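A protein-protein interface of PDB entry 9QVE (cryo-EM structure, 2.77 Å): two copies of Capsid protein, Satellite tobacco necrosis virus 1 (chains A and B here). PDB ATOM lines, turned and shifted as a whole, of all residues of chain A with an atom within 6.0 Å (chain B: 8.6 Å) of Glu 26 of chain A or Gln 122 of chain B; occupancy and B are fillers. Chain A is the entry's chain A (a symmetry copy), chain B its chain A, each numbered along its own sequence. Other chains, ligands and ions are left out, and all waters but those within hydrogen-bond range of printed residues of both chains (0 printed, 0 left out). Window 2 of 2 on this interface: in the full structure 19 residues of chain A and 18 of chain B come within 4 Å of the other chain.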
ATOM      1  N   ASN A  22     -24.814  -3.608   4.564  1.00  0.00           N
ATOM      2  CA  ASN A  22     -24.191  -2.297   4.699  1.00  0.00           C
ATOM      3  C   ASN A  22     -23.557  -1.804   3.406  1.00  0.00           C
ATOM      4  O   ASN A  22     -23.370  -0.592   3.255  1.00  0.00           O
ATOM      5  CB  ASN A  22     -23.136  -2.334   5.804  1.00  0.00           C
ATOM      6  CG  ASN A  22     -23.750  -2.427   7.189  1.00  0.00           C
ATOM      7  OD1 ASN A  22     -23.859  -1.429   7.901  1.00  0.00           O
ATOM      8  ND2 ASN A  22     -24.166  -3.629   7.572  1.00  0.00           N
ATOM      9  N   HIS A  24     -25.084  -1.847   0.656  1.00  0.00           N
ATOM     10  CA  HIS A  24     -26.197  -1.291  -0.097  1.00  0.00           C
ATOM     11  C   HIS A  24     -26.850  -0.108   0.597  1.00  0.00           C
ATOM     12  O   HIS A  24     -27.797   0.467   0.050  1.00  0.00           O
ATOM     13  CB  HIS A  24     -27.249  -2.374  -0.351  1.00  0.00           C
ATOM     14  CG  HIS A  24     -26.761  -3.507  -1.197  1.00  0.00           C
ATOM     15  ND1 HIS A  24     -25.451  -3.617  -1.610  1.00  0.00           N
ATOM     16  CD2 HIS A  24     -27.409  -4.579  -1.710  1.00  0.00           C
ATOM     17  CE1 HIS A  24     -25.312  -4.710  -2.339  1.00  0.00           C
ATOM     18  NE2 HIS A  24     -26.485  -5.311  -2.415  1.00  0.00           N
ATOM     19  N   LEU A  25     -26.378   0.274   1.780  1.00  0.00           N
ATOM     20  CA  LEU A  25     -26.939   1.381   2.538  1.00  0.00           C
ATOM     21  C   LEU A  25     -25.936   2.521   2.582  1.00  0.00           C
ATOM     22  O   LEU A  25     -24.790   2.331   3.005  1.00  0.00           O
ATOM     23  CB  LEU A  25     -27.297   0.947   3.960  1.00  0.00           C
ATOM     24  CG  LEU A  25     -28.218  -0.263   4.107  1.00  0.00           C
ATOM     25  CD1 LEU A  25     -28.506  -0.515   5.569  1.00  0.00           C
ATOM     26  CD2 LEU A  25     -29.505  -0.076   3.338  1.00  0.00           C
ATOM     27  N   GLU A  26     -26.367   3.701   2.149  1.00  0.00           N
ATOM     28  CA  GLU A  26     -25.511   4.874   2.209  1.00  0.00           C
ATOM     29  C   GLU A  26     -25.186   5.216   3.656  1.00  0.00           C
ATOM     30  O   GLU A  26     -26.057   5.190   4.530  1.00  0.00           O
ATOM     31  CB  GLU A  26     -26.195   6.058   1.527  1.00  0.00           C
ATOM     32  CG  GLU A  26     -25.357   7.320   1.462  1.00  0.00           C
ATOM     33  CD  GLU A  26     -26.029   8.422   0.675  1.00  0.00           C
ATOM     34  OE1 GLU A  26     -27.065   8.150   0.034  1.00  0.00           O
ATOM     35  OE2 GLU A  26     -25.521   9.561   0.696  1.00  0.00           O
ATOM     36  N   HIS A  27     -23.916   5.535   3.908  1.00  0.00           N
ATOM     37  CA  HIS A  27     -23.459   5.931   5.238  1.00  0.00           C
ATOM     38  C   HIS A  27     -23.371   7.453   5.269  1.00  0.00           C
ATOM     39  O   HIS A  27     -22.321   8.055   5.041  1.00  0.00           O
ATOM     40  CB  HIS A  27     -22.124   5.276   5.568  1.00  0.00           C
ATOM     41  CG  HIS A  27     -22.239   3.834   5.955  1.00  0.00           C
ATOM     42  ND1 HIS A  27     -22.965   2.922   5.220  1.00  0.00           N
ATOM     43  CD2 HIS A  27     -21.721   3.148   7.001  1.00  0.00           C
ATOM     44  CE1 HIS A  27     -22.888   1.736   5.798  1.00  0.00           C
ATOM     45  NE2 HIS A  27     -22.139   1.845   6.879  1.00  0.00           N
ATOM     46  N   LYS A  28     -24.507   8.078   5.558  1.00  0.00           N
ATOM     47  CA  LYS A  28     -24.569   9.530   5.626  1.00  0.00           C
ATOM     48  C   LYS A  28     -23.721  10.047   6.780  1.00  0.00           C
ATOM     49  O   LYS A  28     -23.536   9.374   7.797  1.00  0.00           O
ATOM     50  CB  LYS A  28     -26.015   9.990   5.787  1.00  0.00           C
ATOM     51  CG  LYS A  28     -26.895   9.714   4.591  1.00  0.00           C
ATOM     52  CD  LYS A  28     -28.272  10.310   4.776  1.00  0.00           C
ATOM     53  CE  LYS A  28     -29.083  10.265   3.493  1.00  0.00           C
ATOM     54  NZ  LYS A  28     -29.338   8.877   3.031  1.00  0.00           N
ATOM     55  N   ARG A  29     -23.200  11.259   6.612  1.00  0.00           N
ATOM     56  CA  ARG A  29     -22.310  11.871   7.586  1.00  0.00           C
ATOM     57  C   ARG A  29     -22.781  13.281   7.904  1.00  0.00           C
ATOM     58  O   ARG A  29     -23.195  14.024   7.011  1.00  0.00           O
ATOM     59  CB  ARG A  29     -20.871  11.902   7.070  1.00  0.00           C
ATOM     60  CG  ARG A  29     -20.293  10.534   6.768  1.00  0.00           C
ATOM     61  CD  ARG A  29     -18.946  10.644   6.088  1.00  0.00           C
ATOM     62  NE  ARG A  29     -17.893  11.031   7.019  1.00  0.00           N
ATOM     63  CZ  ARG A  29     -17.020  10.195   7.563  1.00  0.00           C
ATOM     64  NH1 ARG A  29     -17.025   8.904   7.279  1.00  0.00           N
ATOM     65  NH2 ARG A  29     -16.114  10.668   8.413  1.00  0.00           N
ATOM     66  N   ILE A  58     -27.202  14.854   2.068  1.00  0.00           N
ATOM     67  CA  ILE A  58     -26.354  13.855   2.708  1.00  0.00           C
ATOM     68  C   ILE A  58     -26.305  14.024   4.219  1.00  0.00           C
ATOM     69  O   ILE A  58     -26.051  13.049   4.934  1.00  0.00           O
ATOM     70  CB  ILE A  58     -24.928  13.907   2.141  1.00  0.00           C
ATOM     71  CG1 ILE A  58     -24.153  12.655   2.547  1.00  0.00           C
ATOM     72  CG2 ILE A  58     -24.213  15.144   2.630  1.00  0.00           C
ATOM     73  CD1 ILE A  58     -22.730  12.627   2.058  1.00  0.00           C
ATOM     74  N   TYR A 193     -24.058   7.560   9.933  1.00  0.00           N
ATOM     75  CA  TYR A 193     -25.329   6.899  10.172  1.00  0.00           C
ATOM     76  C   TYR A 193     -25.930   6.421   8.859  1.00  0.00           C
ATOM     77  O   TYR A 193     -25.560   6.878   7.775  1.00  0.00           O
ATOM     78  CB  TYR A 193     -26.314   7.832  10.888  1.00  0.00           C
ATOM     79  CG  TYR A 193     -26.718   9.042  10.085  1.00  0.00           C
ATOM     80  CD1 TYR A 193     -25.988  10.218  10.150  1.00  0.00           C
ATOM     81  CD2 TYR A 193     -27.836   9.014   9.269  1.00  0.00           C
ATOM     82  CE1 TYR A 193     -26.357  11.322   9.422  1.00  0.00           C
ATOM     83  CE2 TYR A 193     -28.211  10.116   8.538  1.00  0.00           C
ATOM     84  CZ  TYR A 193     -27.468  11.268   8.618  1.00  0.00           C
ATOM     85  OH  TYR A 193     -27.842  12.371   7.887  1.00  0.00           O
ATOM     86  N   THR A 194     -26.866   5.484   8.979  1.00  0.00           N
ATOM     87  CA  THR A 194     -27.631   4.964   7.857  1.00  0.00           C
ATOM     88  C   THR A 194     -29.091   5.352   8.026  1.00  0.00           C
ATOM     89  O   THR A 194     -29.652   5.231   9.120  1.00  0.00           O
ATOM     90  CB  THR A 194     -27.516   3.439   7.755  1.00  0.00           C
ATOM     91  OG1 THR A 194     -28.212   2.829   8.847  1.00  0.00           O
ATOM     92  CG2 THR A 194     -26.066   3.007   7.787  1.00  0.00           C
ATOM     93  N   ASP A 195     -29.704   5.819   6.944  1.00  0.00           N
ATOM     94  CA  ASP A 195     -31.106   6.230   6.936  1.00  0.00           C
ATOM     95  C   ASP A 195     -31.839   5.383   5.902  1.00  0.00           C
ATOM     96  O   ASP A 195     -31.934   5.755   4.729  1.00  0.00           O
ATOM     97  CB  ASP A 195     -31.244   7.716   6.644  1.00  0.00           C
ATOM     98  CG  ASP A 195     -32.685   8.169   6.626  1.00  0.00           C
ATOM     99  OD1 ASP A 195     -33.425   7.846   7.578  1.00  0.00           O
ATOM    100  OD2 ASP A 195     -33.077   8.854   5.659  1.00  0.00           O
ATOM    101  N   MET B  95      -7.810  10.010  -5.682  1.00  0.00           N
ATOM    102  CA  MET B  95      -8.525  10.448  -6.874  1.00  0.00           C
ATOM    103  C   MET B  95      -7.897  11.700  -7.471  1.00  0.00           C
ATOM    104  O   MET B  95      -8.574  12.475  -8.149  1.00  0.00           O
ATOM    105  CB  MET B  95      -9.996  10.699  -6.556  1.00  0.00           C
ATOM    106  CG  MET B  95     -10.725   9.481  -6.037  1.00  0.00           C
ATOM    107  SD  MET B  95     -12.399   9.841  -5.496  1.00  0.00           S
ATOM    108  CE  MET B  95     -12.919   8.198  -5.032  1.00  0.00           C
ATOM    109  N   TYR B 116     -13.737  16.079   9.434  1.00  0.00           N
ATOM    110  CA  TYR B 116     -13.463  15.766   8.041  1.00  0.00           C
ATOM    111  C   TYR B 116     -14.700  16.016   7.188  1.00  0.00           C
ATOM    112  O   TYR B 116     -15.835  15.958   7.665  1.00  0.00           O
ATOM    113  CB  TYR B 116     -13.007  14.313   7.904  1.00  0.00           C
ATOM    114  CG  TYR B 116     -11.821  13.959   8.772  1.00  0.00           C
ATOM    115  CD1 TYR B 116     -10.859  14.904   9.088  1.00  0.00           C
ATOM    116  CD2 TYR B 116     -11.667  12.678   9.281  1.00  0.00           C
ATOM    117  CE1 TYR B 116      -9.780  14.585   9.883  1.00  0.00           C
ATOM    118  CE2 TYR B 116     -10.589  12.351  10.078  1.00  0.00           C
ATOM    119  CZ  TYR B 116      -9.649  13.309  10.374  1.00  0.00           C
ATOM    120  OH  TYR B 116      -8.573  12.992  11.168  1.00  0.00           O
ATOM    121  N   ASN B 117     -14.469  16.308   5.916  1.00  0.00           N
ATOM    122  CA  ASN B 117     -15.568  16.629   5.014  1.00  0.00           C
ATOM    123  C   ASN B 117     -16.446  15.400   4.816  1.00  0.00           C
ATOM    124  O   ASN B 117     -15.944  14.356   4.380  1.00  0.00           O
ATOM    125  CB  ASN B 117     -15.033  17.114   3.674  1.00  0.00           C
ATOM    126  CG  ASN B 117     -16.122  17.626   2.763  1.00  0.00           C
ATOM    127  OD1 ASN B 117     -16.838  16.848   2.136  1.00  0.00           O
ATOM    128  ND2 ASN B 117     -16.251  18.940   2.679  1.00  0.00           N
ATOM    129  N   PRO B 118     -17.742  15.466   5.125  1.00  0.00           N
ATOM    130  CA  PRO B 118     -18.588  14.279   4.949  1.00  0.00           C
ATOM    131  C   PRO B 118     -18.702  13.819   3.509  1.00  0.00           C
ATOM    132  O   PRO B 118     -18.788  12.611   3.256  1.00  0.00           O
ATOM    133  CB  PRO B 118     -19.938  14.739   5.509  1.00  0.00           C
ATOM    134  CG  PRO B 118     -19.929  16.194   5.359  1.00  0.00           C
ATOM    135  CD  PRO B 118     -18.524  16.621   5.594  1.00  0.00           C
ATOM    136  N   ILE B 119     -18.710  14.747   2.553  1.00  0.00           N
ATOM    137  CA  ILE B 119     -18.922  14.374   1.158  1.00  0.00           C
ATOM    138  C   ILE B 119     -17.709  13.631   0.611  1.00  0.00           C
ATOM    139  O   ILE B 119     -17.845  12.600  -0.056  1.00  0.00           O
ATOM    140  CB  ILE B 119     -19.250  15.623   0.321  1.00  0.00           C
ATOM    141  CG1 ILE B 119     -20.428  16.372   0.938  1.00  0.00           C
ATOM    142  CG2 ILE B 119     -19.585  15.243  -1.109  1.00  0.00           C
ATOM    143  CD1 ILE B 119     -20.984  17.465   0.062  1.00  0.00           C
ATOM    144  N   THR B 120     -16.507  14.140   0.881  1.00  0.00           N
ATOM    145  CA  THR B 120     -15.305  13.554   0.304  1.00  0.00           C
ATOM    146  C   THR B 120     -14.917  12.232   0.950  1.00  0.00           C
ATOM    147  O   THR B 120     -14.423  11.341   0.251  1.00  0.00           O
ATOM    148  CB  THR B 120     -14.131  14.524   0.420  1.00  0.00           C
ATOM    149  OG1 THR B 120     -13.749  14.658   1.793  1.00  0.00           O
ATOM    150  CG2 THR B 120     -14.507  15.881  -0.134  1.00  0.00           C
ATOM    151  N   LEU B 121     -15.123  12.081   2.257  1.00  0.00           N
ATOM    152  CA  LEU B 121     -14.787  10.835   2.931  1.00  0.00           C
ATOM    153  C   LEU B 121     -15.800   9.734   2.661  1.00  0.00           C
ATOM    154  O   LEU B 121     -15.442   8.552   2.705  1.00  0.00           O
ATOM    155  CB  LEU B 121     -14.669  11.062   4.437  1.00  0.00           C
ATOM    156  CG  LEU B 121     -13.241  11.239   4.949  1.00  0.00           C
ATOM    157  CD1 LEU B 121     -12.598  12.490   4.376  1.00  0.00           C
ATOM    158  CD2 LEU B 121     -13.238  11.276   6.460  1.00  0.00           C
ATOM    159  N   GLN B 122     -17.055  10.093   2.391  1.00  0.00           N
ATOM    160  CA  GLN B 122     -18.014   9.101   1.923  1.00  0.00           C
ATOM    161  C   GLN B 122     -17.560   8.492   0.605  1.00  0.00           C
ATOM    162  O   GLN B 122     -17.635   7.273   0.414  1.00  0.00           O
ATOM    163  CB  GLN B 122     -19.388   9.746   1.767  1.00  0.00           C
ATOM    164  CG  GLN B 122     -20.475   8.795   1.309  1.00  0.00           C
ATOM    165  CD  GLN B 122     -21.728   9.515   0.871  1.00  0.00           C
ATOM    166  OE1 GLN B 122     -21.684  10.393   0.009  1.00  0.00           O
ATOM    167  NE2 GLN B 122     -22.857   9.151   1.467  1.00  0.00           N
ATOM    168  N   GLN B 123     -17.084   9.330  -0.316  1.00  0.00           N
ATOM    169  CA  GLN B 123     -16.557   8.865  -1.590  1.00  0.00           C
ATOM    170  C   GLN B 123     -15.219   8.163  -1.447  1.00  0.00           C
ATOM    171  O   GLN B 123     -14.743   7.570  -2.420  1.00  0.00           O
ATOM    172  CB  GLN B 123     -16.404  10.044  -2.547  1.00  0.00           C
ATOM    173  CG  GLN B 123     -17.663  10.851  -2.747  1.00  0.00           C
ATOM    174  CD  GLN B 123     -17.395  12.186  -3.392  1.00  0.00           C
ATOM    175  OE1 GLN B 123     -16.307  12.432  -3.912  1.00  0.00           O
ATOM    176  NE2 GLN B 123     -18.385  13.063  -3.355  1.00  0.00           N
ATOM    177  N   LYS B 124     -14.605   8.218  -0.267  1.00  0.00           N
ATOM    178  CA  LYS B 124     -13.251   7.718  -0.059  1.00  0.00           C
ATOM    179  C   LYS B 124     -12.256   8.456  -0.945  1.00  0.00           C
ATOM    180  O   LYS B 124     -11.257   7.887  -1.391  1.00  0.00           O
ATOM    181  CB  LYS B 124     -13.179   6.210  -0.296  1.00  0.00           C
ATOM    182  CG  LYS B 124     -14.158   5.434   0.559  1.00  0.00           C
ATOM    183  CD  LYS B 124     -14.058   3.944   0.329  1.00  0.00           C
ATOM    184  CE  LYS B 124     -15.079   3.194   1.163  1.00  0.00           C
ATOM    185  NZ  LYS B 124     -14.963   3.511   2.612  1.00  0.00           N
ATOM    186  N   ARG B 125     -12.530   9.737  -1.200  1.00  0.00           N
ATOM    187  CA  ARG B 125     -11.603  10.554  -1.971  1.00  0.00           C
ATOM    188  C   ARG B 125     -10.262  10.661  -1.264  1.00  0.00           C
ATOM    189  O   ARG B 125      -9.205  10.580  -1.900  1.00  0.00           O
ATOM    190  CB  ARG B 125     -12.197  11.942  -2.197  1.00  0.00           C
ATOM    191  CG  ARG B 125     -11.421  12.790  -3.182  1.00  0.00           C
ATOM    192  CD  ARG B 125     -12.321  13.360  -4.259  1.00  0.00           C
ATOM    193  NE  ARG B 125     -12.940  14.613  -3.852  1.00  0.00           N
ATOM    194  CZ  ARG B 125     -14.058  15.100  -4.373  1.00  0.00           C
ATOM    195  NH1 ARG B 125     -14.742  14.435  -5.289  1.00  0.00           N
ATOM    196  NH2 ARG B 125     -14.505  16.281  -3.957  1.00  0.00           N
ATOM    197  N   PHE B 126     -10.289  10.841   0.051  1.00  0.00           N
ATOM    198  CA  PHE B 126      -9.093  10.898   0.871  1.00  0.00           C
ATOM    199  C   PHE B 126      -9.121   9.761   1.880  1.00  0.00           C
ATOM    200  O   PHE B 126     -10.186   9.352   2.351  1.00  0.00           O
ATOM    201  CB  PHE B 126      -8.978  12.233   1.608  1.00  0.00           C
ATOM    202  CG  PHE B 126      -9.237  13.432   0.746  1.00  0.00           C
ATOM    203  CD1 PHE B 126      -8.243  13.947  -0.060  1.00  0.00           C
ATOM    204  CD2 PHE B 126     -10.472  14.050   0.752  1.00  0.00           C
ATOM    205  CE1 PHE B 126      -8.476  15.050  -0.847  1.00  0.00           C
ATOM    206  CE2 PHE B 126     -10.709  15.155  -0.037  1.00  0.00           C
ATOM    207  CZ  PHE B 126      -9.709  15.656  -0.837  1.00  0.00           C
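Of the 11 printed residues of chain A, 4 touch a printed residue of chain B.
Of the 12 printed residues of chain B, 3 touch a printed residue of chain A.
Hydrophobic or aromatic side chains of chain B within 4 Å of the printed part of chain A: Pro 118 and Leu 121.
Along chain B the printed residues that touch a printed residue of chain A span positions 118 to 122.
Among the printed residues, no Asp or Glu carboxylate lies within 4 Å of a Lys or Arg side-chain nitrogen of the other chain.
The side-chain amide nitrogen (NE2) of Gln 122 of chain B sits at hydrogen-bond distance from the side-chain carboxylate (OE2) of Glu 26 of chain A, at 2.8 Å.
His 27 of chain A touches Gln 122 of chain B.
Pro 118 of chain B touches Arg 29 of chain A.
CD2 of Leu 121 of chain B touches NH2 of Arg 29 of chain A, 3.5 Å away.
Ile 58 of chain A touches Gln 122 of chain B (CD1 to OE1, 3.2 Å).
No position is printed for both chains.
O of Leu 25 of chain A lies within hydrogen-bond range of ND1 of His 27 of chain A.
OE1 of Glu 26 of chain A lies close to NZ of Lys 28 of chain A, at 3.8 Å.
Printed residues of chain B within 4 Å of Glu 26 of chain A: Gln 122.
Printed residues of chain A within 4 Å of Gln 122 of chain B: Glu 26 (2.8 Å), His 27 (3.8 Å) and Ile 58 (3.2 Å).
Of the printed residues of chain A, Pro 118 of chain B touches Arg 29.
Printed residues of chain B within 4 Å of Arg 29 of chain A: Pro 118 and Leu 121.
Of the printed residues of chain B, Ile 58 of chain A touches Gln 122 (3.2 Å).
The nearest printed residue of chain B that does not touch His 27 of chain A is Pro 118 of chain B (6.0 Å).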
